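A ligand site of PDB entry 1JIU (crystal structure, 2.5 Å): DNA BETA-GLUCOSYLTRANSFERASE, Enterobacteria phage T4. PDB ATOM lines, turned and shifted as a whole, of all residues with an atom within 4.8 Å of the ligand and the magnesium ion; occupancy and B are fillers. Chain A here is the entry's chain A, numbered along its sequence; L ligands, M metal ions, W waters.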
ATOM      1  N   VAL A  18     -23.257  -1.156   2.763  1.00  0.00           N
ATOM      2  CA  VAL A  18     -22.819  -2.414   2.176  1.00  0.00           C
ATOM      3  C   VAL A  18     -21.308  -2.610   2.083  1.00  0.00           C
ATOM      4  O   VAL A  18     -20.811  -3.694   2.400  1.00  0.00           O
ATOM      5  CB  VAL A  18     -23.424  -2.591   0.791  1.00  0.00           C
ATOM      6  CG1 VAL A  18     -22.946  -3.905   0.180  1.00  0.00           C
ATOM      7  CG2 VAL A  18     -24.934  -2.566   0.892  1.00  0.00           C
ATOM      8  N   THR A  99     -14.898  -8.418  -6.459  1.00  0.00           N
ATOM      9  CA  THR A  99     -16.227  -8.994  -6.287  1.00  0.00           C
ATOM     10  C   THR A  99     -17.345  -8.306  -7.072  1.00  0.00           C
ATOM     11  O   THR A  99     -18.464  -8.809  -7.121  1.00  0.00           O
ATOM     12  CB  THR A  99     -16.645  -8.969  -4.801  1.00  0.00           C
ATOM     13  OG1 THR A  99     -16.621  -7.619  -4.333  1.00  0.00           O
ATOM     14  CG2 THR A  99     -15.704  -9.835  -3.967  1.00  0.00           C
ATOM     15  N   ASP A 100     -17.030  -7.150  -7.657  1.00  0.00           N
ATOM     16  CA  ASP A 100     -18.007  -6.397  -8.438  1.00  0.00           C
ATOM     17  C   ASP A 100     -17.379  -6.115  -9.801  1.00  0.00           C
ATOM     18  O   ASP A 100     -16.302  -5.526  -9.892  1.00  0.00           O
ATOM     19  CB  ASP A 100     -18.378  -5.097  -7.721  1.00  0.00           C
ATOM     20  CG  ASP A 100     -19.523  -4.348  -8.394  1.00  0.00           C
ATOM     21  OD1 ASP A 100     -20.263  -3.623  -7.691  1.00  0.00           O
ATOM     22  OD2 ASP A 100     -19.698  -4.462  -9.628  1.00  0.00           O
ATOM     23  N   GLU A 163     -17.554 -14.466  -2.124  1.00  0.00           N
ATOM     24  CA  GLU A 163     -18.819 -14.259  -1.443  1.00  0.00           C
ATOM     25  C   GLU A 163     -19.535 -15.469  -0.832  1.00  0.00           C
ATOM     26  O   GLU A 163     -20.694 -15.382  -0.425  1.00  0.00           O
ATOM     27  CB  GLU A 163     -19.742 -13.461  -2.367  1.00  0.00           C
ATOM     28  CG  GLU A 163     -19.024 -12.227  -2.918  1.00  0.00           C
ATOM     29  CD  GLU A 163     -19.936 -11.079  -3.263  1.00  0.00           C
ATOM     30  OE1 GLU A 163     -20.932 -11.288  -3.994  1.00  0.00           O
ATOM     31  OE2 GLU A 163     -19.657  -9.941  -2.826  1.00  0.00           O
ATOM     32  N   TYR A 186     -36.672  -8.377  -4.188  1.00  0.00           N
ATOM     33  CA  TYR A 186     -35.318  -8.169  -4.691  1.00  0.00           C
ATOM     34  C   TYR A 186     -34.740  -6.984  -3.940  1.00  0.00           C
ATOM     35  O   TYR A 186     -35.394  -5.952  -3.783  1.00  0.00           O
ATOM     36  CB  TYR A 186     -35.333  -7.885  -6.193  1.00  0.00           C
ATOM     37  CG  TYR A 186     -33.974  -7.532  -6.775  1.00  0.00           C
ATOM     38  CD1 TYR A 186     -33.529  -6.211  -6.790  1.00  0.00           C
ATOM     39  CD2 TYR A 186     -33.123  -8.518  -7.280  1.00  0.00           C
ATOM     40  CE1 TYR A 186     -32.272  -5.881  -7.293  1.00  0.00           C
ATOM     41  CE2 TYR A 186     -31.868  -8.198  -7.783  1.00  0.00           C
ATOM     42  CZ  TYR A 186     -31.451  -6.873  -7.783  1.00  0.00           C
ATOM     43  OH  TYR A 186     -30.199  -6.541  -8.255  1.00  0.00           O
ATOM     44  N   GLY A 187     -33.502  -7.141  -3.463  1.00  0.00           N
ATOM     45  CA  GLY A 187     -32.840  -6.068  -2.740  1.00  0.00           C
ATOM     46  C   GLY A 187     -31.461  -5.745  -3.303  1.00  0.00           C
ATOM     47  O   GLY A 187     -30.626  -6.626  -3.466  1.00  0.00           O
ATOM     48  N   GLY A 188     -31.232  -4.481  -3.615  1.00  0.00           N
ATOM     49  CA  GLY A 188     -29.951  -4.066  -4.156  1.00  0.00           C
ATOM     50  C   GLY A 188     -30.027  -2.611  -4.550  1.00  0.00           C
ATOM     51  O   GLY A 188     -31.063  -1.978  -4.362  1.00  0.00           O
ATOM     52  N   SER A 189     -28.946  -2.073  -5.096  1.00  0.00           N
ATOM     53  CA  SER A 189     -28.951  -0.669  -5.518  1.00  0.00           C
ATOM     54  C   SER A 189     -29.352  -0.571  -6.990  1.00  0.00           C
ATOM     55  O   SER A 189     -29.713  -1.570  -7.603  1.00  0.00           O
ATOM     56  CB  SER A 189     -27.577  -0.023  -5.316  1.00  0.00           C
ATOM     57  OG  SER A 189     -26.553  -0.745  -5.963  1.00  0.00           O
ATOM     58  N   ARG A 191     -27.369   0.204  -9.265  1.00  0.00           N
ATOM     59  CA  ARG A 191     -26.179  -0.211 -10.005  1.00  0.00           C
ATOM     60  C   ARG A 191     -25.956   0.746 -11.162  1.00  0.00           C
ATOM     61  O   ARG A 191     -25.487   0.350 -12.223  1.00  0.00           O
ATOM     62  CB  ARG A 191     -26.324  -1.641 -10.530  1.00  0.00           C
ATOM     63  CG  ARG A 191     -26.159  -2.676  -9.442  1.00  0.00           C
ATOM     64  CD  ARG A 191     -25.761  -4.020 -10.018  1.00  0.00           C
ATOM     65  NE  ARG A 191     -24.433  -4.020 -10.659  1.00  0.00           N
ATOM     66  CZ  ARG A 191     -23.277  -3.985 -10.006  1.00  0.00           C
ATOM     67  NH1 ARG A 191     -23.239  -3.941  -8.685  1.00  0.00           N
ATOM     68  NH2 ARG A 191     -22.143  -4.016 -10.685  1.00  0.00           N
ATOM     69  N   ARG A 195     -28.192  -2.592 -14.908  1.00  0.00           N
ATOM     70  CA  ARG A 195     -29.066  -3.754 -14.892  1.00  0.00           C
ATOM     71  C   ARG A 195     -30.525  -3.362 -14.949  1.00  0.00           C
ATOM     72  O   ARG A 195     -31.384  -4.067 -14.411  1.00  0.00           O
ATOM     73  CB  ARG A 195     -28.767  -4.528 -13.605  1.00  0.00           C
ATOM     74  CG  ARG A 195     -29.306  -5.945 -13.530  1.00  0.00           C
ATOM     75  CD  ARG A 195     -29.010  -6.531 -12.149  1.00  0.00           C
ATOM     76  NE  ARG A 195     -27.576  -6.592 -11.861  1.00  0.00           N
ATOM     77  CZ  ARG A 195     -27.051  -7.018 -10.708  1.00  0.00           C
ATOM     78  NH1 ARG A 195     -27.834  -7.428  -9.720  1.00  0.00           N
ATOM     79  NH2 ARG A 195     -25.735  -7.044 -10.554  1.00  0.00           N
ATOM     80  N   PHE A 213     -36.279  -3.652  -2.241  1.00  0.00           N
ATOM     81  CA  PHE A 213     -35.642  -2.914  -1.153  1.00  0.00           C
ATOM     82  C   PHE A 213     -34.229  -2.567  -1.581  1.00  0.00           C
ATOM     83  O   PHE A 213     -33.765  -3.041  -2.616  1.00  0.00           O
ATOM     84  CB  PHE A 213     -35.663  -3.690   0.176  1.00  0.00           C
ATOM     85  CG  PHE A 213     -34.916  -5.004   0.181  1.00  0.00           C
ATOM     86  CD1 PHE A 213     -35.472  -6.141  -0.404  1.00  0.00           C
ATOM     87  CD2 PHE A 213     -33.705  -5.125   0.853  1.00  0.00           C
ATOM     88  CE1 PHE A 213     -34.843  -7.374  -0.304  1.00  0.00           C
ATOM     89  CE2 PHE A 213     -33.063  -6.350   0.961  1.00  0.00           C
ATOM     90  CZ  PHE A 213     -33.628  -7.484   0.388  1.00  0.00           C
ATOM     91  N   GLY A 214     -33.556  -1.733  -0.797  1.00  0.00           N
ATOM     92  CA  GLY A 214     -32.204  -1.332  -1.137  1.00  0.00           C
ATOM     93  C   GLY A 214     -32.085   0.145  -1.471  1.00  0.00           C
ATOM     94  O   GLY A 214     -33.016   0.920  -1.247  1.00  0.00           O
ATOM     95  N   GLY A 236     -36.564   1.249   0.588  1.00  0.00           N
ATOM     96  CA  GLY A 236     -35.316   1.703   1.176  1.00  0.00           C
ATOM     97  C   GLY A 236     -34.360   0.617   1.622  1.00  0.00           C
ATOM     98  O   GLY A 236     -34.685  -0.570   1.580  1.00  0.00           O
ATOM     99  N   LYS A 237     -33.188   1.040   2.071  1.00  0.00           N
ATOM    100  CA  LYS A 237     -32.137   0.136   2.523  1.00  0.00           C
ATOM    101  C   LYS A 237     -32.332  -0.414   3.930  1.00  0.00           C
ATOM    102  O   LYS A 237     -33.128   0.100   4.703  1.00  0.00           O
ATOM    103  CB  LYS A 237     -30.801   0.870   2.474  1.00  0.00           C
ATOM    104  CG  LYS A 237     -30.657   1.925   3.556  1.00  0.00           C
ATOM    105  CD  LYS A 237     -29.429   2.821   3.334  1.00  0.00           C
ATOM    106  CE  LYS A 237     -28.135   2.033   3.366  1.00  0.00           C
ATOM    107  NZ  LYS A 237     -26.959   2.888   3.043  1.00  0.00           N
ATOM    108  N   ILE A 238     -31.603  -1.485   4.220  1.00  0.00           N
ATOM    109  CA  ILE A 238     -31.608  -2.122   5.540  1.00  0.00           C
ATOM    110  C   ILE A 238     -30.191  -2.644   5.691  1.00  0.00           C
ATOM    111  O   ILE A 238     -29.444  -2.712   4.712  1.00  0.00           O
ATOM    112  CB  ILE A 238     -32.596  -3.316   5.636  1.00  0.00           C
ATOM    113  CG1 ILE A 238     -32.200  -4.424   4.662  1.00  0.00           C
ATOM    114  CG2 ILE A 238     -34.020  -2.839   5.407  1.00  0.00           C
ATOM    115  CD1 ILE A 238     -32.870  -5.762   4.948  1.00  0.00           C
ATOM    116  N   PRO A 239     -29.791  -3.010   6.912  1.00  0.00           N
ATOM    117  CA  PRO A 239     -28.432  -3.521   7.133  1.00  0.00           C
ATOM    118  C   PRO A 239     -28.189  -4.848   6.398  1.00  0.00           C
ATOM    119  O   PRO A 239     -29.071  -5.712   6.329  1.00  0.00           O
ATOM    120  CB  PRO A 239     -28.370  -3.679   8.642  1.00  0.00           C
ATOM    121  CG  PRO A 239     -29.316  -2.632   9.139  1.00  0.00           C
ATOM    122  CD  PRO A 239     -30.471  -2.788   8.197  1.00  0.00           C
ATOM    123  N   MET A 240     -26.977  -5.009   5.865  1.00  0.00           N
ATOM    124  CA  MET A 240     -26.634  -6.234   5.169  1.00  0.00           C
ATOM    125  C   MET A 240     -26.941  -7.475   6.010  1.00  0.00           C
ATOM    126  O   MET A 240     -27.429  -8.473   5.488  1.00  0.00           O
ATOM    127  CB  MET A 240     -25.160  -6.245   4.759  1.00  0.00           C
ATOM    128  CG  MET A 240     -24.743  -7.519   4.054  1.00  0.00           C
ATOM    129  SD  MET A 240     -23.045  -7.476   3.463  1.00  0.00           S
ATOM    130  CE  MET A 240     -22.625  -9.203   3.530  1.00  0.00           C
ATOM    131  N   VAL A 243     -30.483  -8.920   5.608  1.00  0.00           N
ATOM    132  CA  VAL A 243     -30.938  -9.271   4.269  1.00  0.00           C
ATOM    133  C   VAL A 243     -31.717 -10.586   4.104  1.00  0.00           C
ATOM    134  O   VAL A 243     -32.695 -10.628   3.351  1.00  0.00           O
ATOM    135  CB  VAL A 243     -29.757  -9.277   3.287  1.00  0.00           C
ATOM    136  CG1 VAL A 243     -30.204  -9.792   1.934  1.00  0.00           C
ATOM    137  CG2 VAL A 243     -29.197  -7.876   3.159  1.00  0.00           C
ATOM    138  N   ILE A 256     -30.577 -11.897 -10.265  1.00  0.00           N
ATOM    139  CA  ILE A 256     -30.184 -11.373 -11.561  1.00  0.00           C
ATOM    140  C   ILE A 256     -28.837 -10.694 -11.366  1.00  0.00           C
ATOM    141  O   ILE A 256     -28.441 -10.410 -10.227  1.00  0.00           O
ATOM    142  CB  ILE A 256     -31.168 -10.310 -12.103  1.00  0.00           C
ATOM    143  CG1 ILE A 256     -31.444  -9.260 -11.035  1.00  0.00           C
ATOM    144  CG2 ILE A 256     -32.439 -10.987 -12.595  1.00  0.00           C
ATOM    145  CD1 ILE A 256     -32.231  -8.065 -11.533  1.00  0.00           C
ATOM    146  N   ASP A 258     -25.315  -8.384 -13.610  1.00  0.00           N
ATOM    147  CA  ASP A 258     -24.882  -7.571 -14.744  1.00  0.00           C
ATOM    148  C   ASP A 258     -24.591  -8.539 -15.910  1.00  0.00           C
ATOM    149  O   ASP A 258     -24.472  -9.739 -15.708  1.00  0.00           O
ATOM    150  CB  ASP A 258     -23.609  -6.792 -14.379  1.00  0.00           C
ATOM    151  CG  ASP A 258     -23.895  -5.563 -13.520  1.00  0.00           C
ATOM    152  OD1 ASP A 258     -24.874  -5.552 -12.744  1.00  0.00           O
ATOM    153  OD2 ASP A 258     -23.120  -4.588 -13.632  1.00  0.00           O
ATOM    154  N   TYR A 261     -21.725 -10.776 -15.452  1.00  0.00           N
ATOM    155  CA  TYR A 261     -21.840 -11.589 -14.238  1.00  0.00           C
ATOM    156  C   TYR A 261     -22.227 -12.989 -14.706  1.00  0.00           C
ATOM    157  O   TYR A 261     -21.784 -13.990 -14.150  1.00  0.00           O
ATOM    158  CB  TYR A 261     -22.959 -11.060 -13.332  1.00  0.00           C
ATOM    159  CG  TYR A 261     -22.557 -10.094 -12.228  1.00  0.00           C
ATOM    160  CD1 TYR A 261     -21.650  -9.061 -12.455  1.00  0.00           C
ATOM    161  CD2 TYR A 261     -23.156 -10.174 -10.971  1.00  0.00           C
ATOM    162  CE1 TYR A 261     -21.341  -8.132 -11.465  1.00  0.00           C
ATOM    163  CE2 TYR A 261     -22.857  -9.254  -9.969  1.00  0.00           C
ATOM    164  CZ  TYR A 261     -21.957  -8.242 -10.224  1.00  0.00           C
ATOM    165  OH  TYR A 261     -21.659  -7.331  -9.222  1.00  0.00           O
ATOM    166  N   THR A 267     -22.690 -14.631  -7.157  1.00  0.00           N
ATOM    167  CA  THR A 267     -22.762 -13.568  -6.163  1.00  0.00           C
ATOM    168  C   THR A 267     -23.307 -13.878  -4.772  1.00  0.00           C
ATOM    169  O   THR A 267     -23.815 -14.962  -4.495  1.00  0.00           O
ATOM    170  CB  THR A 267     -23.560 -12.386  -6.721  1.00  0.00           C
ATOM    171  OG1 THR A 267     -24.880 -12.816  -7.064  1.00  0.00           O
ATOM    172  CG2 THR A 267     -22.872 -11.841  -7.964  1.00  0.00           C
ATOM    173  N   LEU A 268     -23.212 -12.872  -3.903  1.00  0.00           N
ATOM    174  CA  LEU A 268     -23.649 -12.952  -2.521  1.00  0.00           C
ATOM    175  C   LEU A 268     -25.159 -13.127  -2.390  1.00  0.00           C
ATOM    176  O   LEU A 268     -25.624 -13.865  -1.528  1.00  0.00           O
ATOM    177  CB  LEU A 268     -23.194 -11.702  -1.763  1.00  0.00           C
ATOM    178  CG  LEU A 268     -23.500 -11.608  -0.268  1.00  0.00           C
ATOM    179  CD1 LEU A 268     -22.803 -12.724   0.506  1.00  0.00           C
ATOM    180  CD2 LEU A 268     -23.041 -10.264   0.252  1.00  0.00           C
ATOM    181  N   ARG A 269     -25.931 -12.442  -3.241  1.00  0.00           N
ATOM    182  CA  ARG A 269     -27.384 -12.558  -3.184  1.00  0.00           C
ATOM    183  C   ARG A 269     -27.867 -13.985  -3.462  1.00  0.00           C
ATOM    184  O   ARG A 269     -28.984 -14.348  -3.081  1.00  0.00           O
ATOM    185  CB  ARG A 269     -28.063 -11.600  -4.175  1.00  0.00           C
ATOM    186  CG  ARG A 269     -27.875 -11.951  -5.639  1.00  0.00           C
ATOM    187  CD  ARG A 269     -28.817 -11.160  -6.549  1.00  0.00           C
ATOM    188  NE  ARG A 269     -28.629  -9.705  -6.488  1.00  0.00           N
ATOM    189  CZ  ARG A 269     -29.197  -8.906  -5.594  1.00  0.00           C
ATOM    190  NH1 ARG A 269     -30.023  -9.407  -4.675  1.00  0.00           N
ATOM    191  NH2 ARG A 269     -28.938  -7.604  -5.608  1.00  0.00           N
ATOM    192  N   GLU A 272     -27.691 -15.466   0.010  1.00  0.00           N
ATOM    193  CA  GLU A 272     -28.643 -14.796   0.902  1.00  0.00           C
ATOM    194  C   GLU A 272     -30.062 -15.214   0.563  1.00  0.00           C
ATOM    195  O   GLU A 272     -30.946 -15.218   1.437  1.00  0.00           O
ATOM    196  CB  GLU A 272     -28.562 -13.282   0.754  1.00  0.00           C
ATOM    197  CG  GLU A 272     -27.221 -12.644   1.074  1.00  0.00           C
ATOM    198  CD  GLU A 272     -27.203 -11.203   0.646  1.00  0.00           C
ATOM    199  OE1 GLU A 272     -27.660 -10.924  -0.480  1.00  0.00           O
ATOM    200  OE2 GLU A 272     -26.732 -10.346   1.421  1.00  0.00           O
HETATM  201  N1  LIG L   1     -27.953  -5.181   0.453  1.00  0.00           N
HETATM  202  C1  LIG L   1     -28.035  -4.653   1.739  1.00  0.00           C
HETATM  203  N2  LIG L   1     -29.169  -3.914   1.987  1.00  0.00           N
HETATM  204  C2  LIG L   1     -30.189  -3.655   1.126  1.00  0.00           C
HETATM  205  C3  LIG L   1     -30.055  -4.251  -0.165  1.00  0.00           C
HETATM  206  C4  LIG L   1     -28.966  -4.968  -0.458  1.00  0.00           C
HETATM  207  O1  LIG L   1     -27.181  -4.824   2.573  1.00  0.00           O
HETATM  208  O2  LIG L   1     -31.090  -2.885   1.477  1.00  0.00           O
HETATM  209  C5  LIG L   1     -26.745  -5.945   0.102  1.00  0.00           C
HETATM  210  C6  LIG L   1     -26.906  -7.472   0.071  1.00  0.00           C
HETATM  211  O3  LIG L   1     -25.719  -8.076   0.578  1.00  0.00           O
HETATM  212  C7  LIG L   1     -27.128  -7.728  -1.412  1.00  0.00           C
HETATM  213  C8  LIG L   1     -26.246  -6.681  -2.072  1.00  0.00           C
HETATM  214  O4  LIG L   1     -26.303  -5.536  -1.176  1.00  0.00           O
HETATM  215  O5  LIG L   1     -26.718  -9.022  -1.821  1.00  0.00           O
HETATM  216  C9  LIG L   1     -26.685  -6.261  -3.452  1.00  0.00           C
HETATM  217  O6  LIG L   1     -25.607  -5.609  -4.114  1.00  0.00           O
HETATM  218  P1  LIG L   1     -25.822  -4.955  -5.551  1.00  0.00           P
HETATM  219  O7  LIG L   1     -27.033  -4.089  -5.499  1.00  0.00           O
HETATM  220  O8  LIG L   1     -24.531  -4.371  -5.971  1.00  0.00           O
HETATM  221  O9  LIG L   1     -26.128  -6.221  -6.454  1.00  0.00           O
HETATM  222  P2  LIG L   1     -25.136  -7.274  -7.111  1.00  0.00           P
HETATM  223  O10 LIG L   1     -24.446  -6.398  -8.087  1.00  0.00           O
HETATM  224  O11 LIG L   1     -26.099  -8.263  -7.678  1.00  0.00           O
HETATM  225  O12 LIG L   1     -24.336  -7.729  -5.940  1.00  0.00           O
HETATM  226 MG    MG M   1     -22.306  -7.355  -4.786  1.00  0.00          MG
HETATM  227  O   HOH W   1     -26.098 -10.769  -8.509  1.00  0.00           O
HETATM  228  O   HOH W   2     -28.785  -1.453  -1.734  1.00  0.00           O
HETATM  229  O   HOH W   3     -26.674  -3.056  -2.565  1.00  0.00           O
HETATM  230  O   HOH W   4     -21.354  -8.501  -6.608  1.00  0.00           O
HETATM  231  O   HOH W   5     -25.153  -9.644  -3.980  1.00  0.00           O
HETATM  232  O   HOH W   6     -28.979  -4.011  -7.582  1.00  0.00           O
HETATM  233  O   HOH W   7     -20.198  -7.505  -4.551  1.00  0.00           O
HETATM  234  O   HOH W   8     -22.600  -9.251  -4.524  1.00  0.00           O
HETATM  235  O   HOH W   9     -25.527  -2.596   4.570  1.00  0.00           O
HETATM  236  O   HOH W  10     -22.180  -6.292  -6.318  1.00  0.00           O
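An oxygen (O7) of the ligand is in hydrogen-bond range of the backbone NH of Ser 189 (2.8 Å).
An oxygen (O11) of the ligand lies within salt-bridge range of the guanidinium group of Arg 269, 3.1 Å away.
N2 of the ligand sits at hydrogen-bond distance from O of Ile 238 (3.0 Å).
An oxygen (O10) of the ligand is in hydrogen-bond range of the side-chain hydroxyl of Tyr 261, at 3.2 Å.
N of Ile 238 is in hydrogen-bond range of O2 of the ligand (3.1 Å).
An oxygen (O5) of the ligand is in hydrogen-bond range of the side-chain carboxylate (OE1) of Glu 272 (2.5 Å).
An oxygen (O7) of the ligand is in hydrogen-bond range of the side-chain hydroxyl of Ser 189 (3.4 Å).
NH1 of Arg 191 is in salt-bridge range of O10 of the ligand, 2.8 Å away.
The guanidinium group (NH1) of Arg 195 is in salt-bridge range of an oxygen (O11) of the ligand, at 2.8 Å.
The backbone NH (N) of Met 240 sits close to an oxygen (O1) of the ligand, at 3.3 Å.
NH1 of Arg 195 is in hydrogen-bond range of O of Ile 256 (3.1 Å).
The side-chain carboxylate (OE1) of Glu 163 lies within hydrogen-bond range of the backbone NH (N) of Leu 268 (2.8 Å).
The backbone carbonyl oxygen (O) of Gly 236 sits at hydrogen-bond distance from the backbone NH (N) of Gly 214 (2.9 Å).
The guanidinium group of Arg 195 lies within hydrogen-bond range of the side-chain hydroxyl of Tyr 186 (2.9 Å).
NE of Arg 191 is in salt-bridge range of OD1 of Asp 258, at 2.6 Å.
The side-chain carboxylate (OD2) of Asp 100 lies within salt-bridge range of the guanidinium group (NH2) of Arg 191 (2.7 Å).
The guanidinium group (NH2) of Arg 269 lies within hydrogen-bond range of the backbone carbonyl oxygen (O) of Gly 187 (2.9 Å).
The backbone NH of Gly 188 is in hydrogen-bond range of the backbone carbonyl oxygen of Phe 213, 3.1 Å away.
Val 18 touches the ligand.
C of Gly 187 touches C3 of the ligand, 3.7 Å away.
Gly 188 touches the ligand (CA to O7, 3.2 Å).
Phe 213 touches the ligand (CD2 to O2, 3.5 Å).
CA of Gly 214 touches O2 of the ligand, 3.2 Å away.
Lys 237 touches the ligand (CA to O2, 3.4 Å).
Pro 239 touches the ligand.
CG2 of Val 243 touches O1 of the ligand, 3.7 Å away.
Leu 268 touches the ligand (CD2 to O3, 3.5 Å).
Hydrophobic or aromatic side chains that line the ligand: Val 18, Phe 213, Ile 238, Met 240, Val 243, Tyr 261 and Leu 268.
Within 4 Å of the ligand: Val 18, Gly 187, Gly 188, Ser 189, Arg 191, Arg 195, Phe 213, Gly 214, Lys 237, Ile 238, Pro 239, Met 240, Val 243, Tyr 261, Leu 268, Arg 269 and Glu 272.
The nearest printed residue that does not touch the ligand is Ile 256 (4.1 Å).
No residue comes within 4 Å of the magnesium ion.
The nearest printed residue that does not touch the magnesium ion is Glu 163 (4.2 Å).
The magnesium ion is bound by water W10, water W8, water W7, water W4 and O12 of the ligand.
The magnesium ion has five donor atoms within binding distance.
Water W10 bridges an oxygen (O10) of the ligand and the side-chain hydroxyl (OH) of Tyr 261.
Water W4 bridges the side-chain hydroxyl of Tyr 261 (2.9 Å) and the backbone carbonyl oxygen of Thr 99 (3.0 Å).
Water W7 lies within hydrogen-bond range of the side-chain carboxylate (OE2) of Glu 163 (3.0 Å) and the backbone carbonyl oxygen (O) of Thr 99 (3.4 Å).
Water W5 lies within hydrogen-bond range of an oxygen (O5) of the ligand and the backbone NH of Arg 269.
Water W6 lies within hydrogen-bond range of the backbone carbonyl oxygen (O) of Ser 189 (2.5 Å), an oxygen (O7) of the ligand (2.9 Å) and the side-chain hydroxyl (OH) of Tyr 186 (2.9 Å).
Water W9 lies within hydrogen-bond range of the backbone NH of Met 240, the backbone NH of Val 18 and an oxygen (O1) of the ligand.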
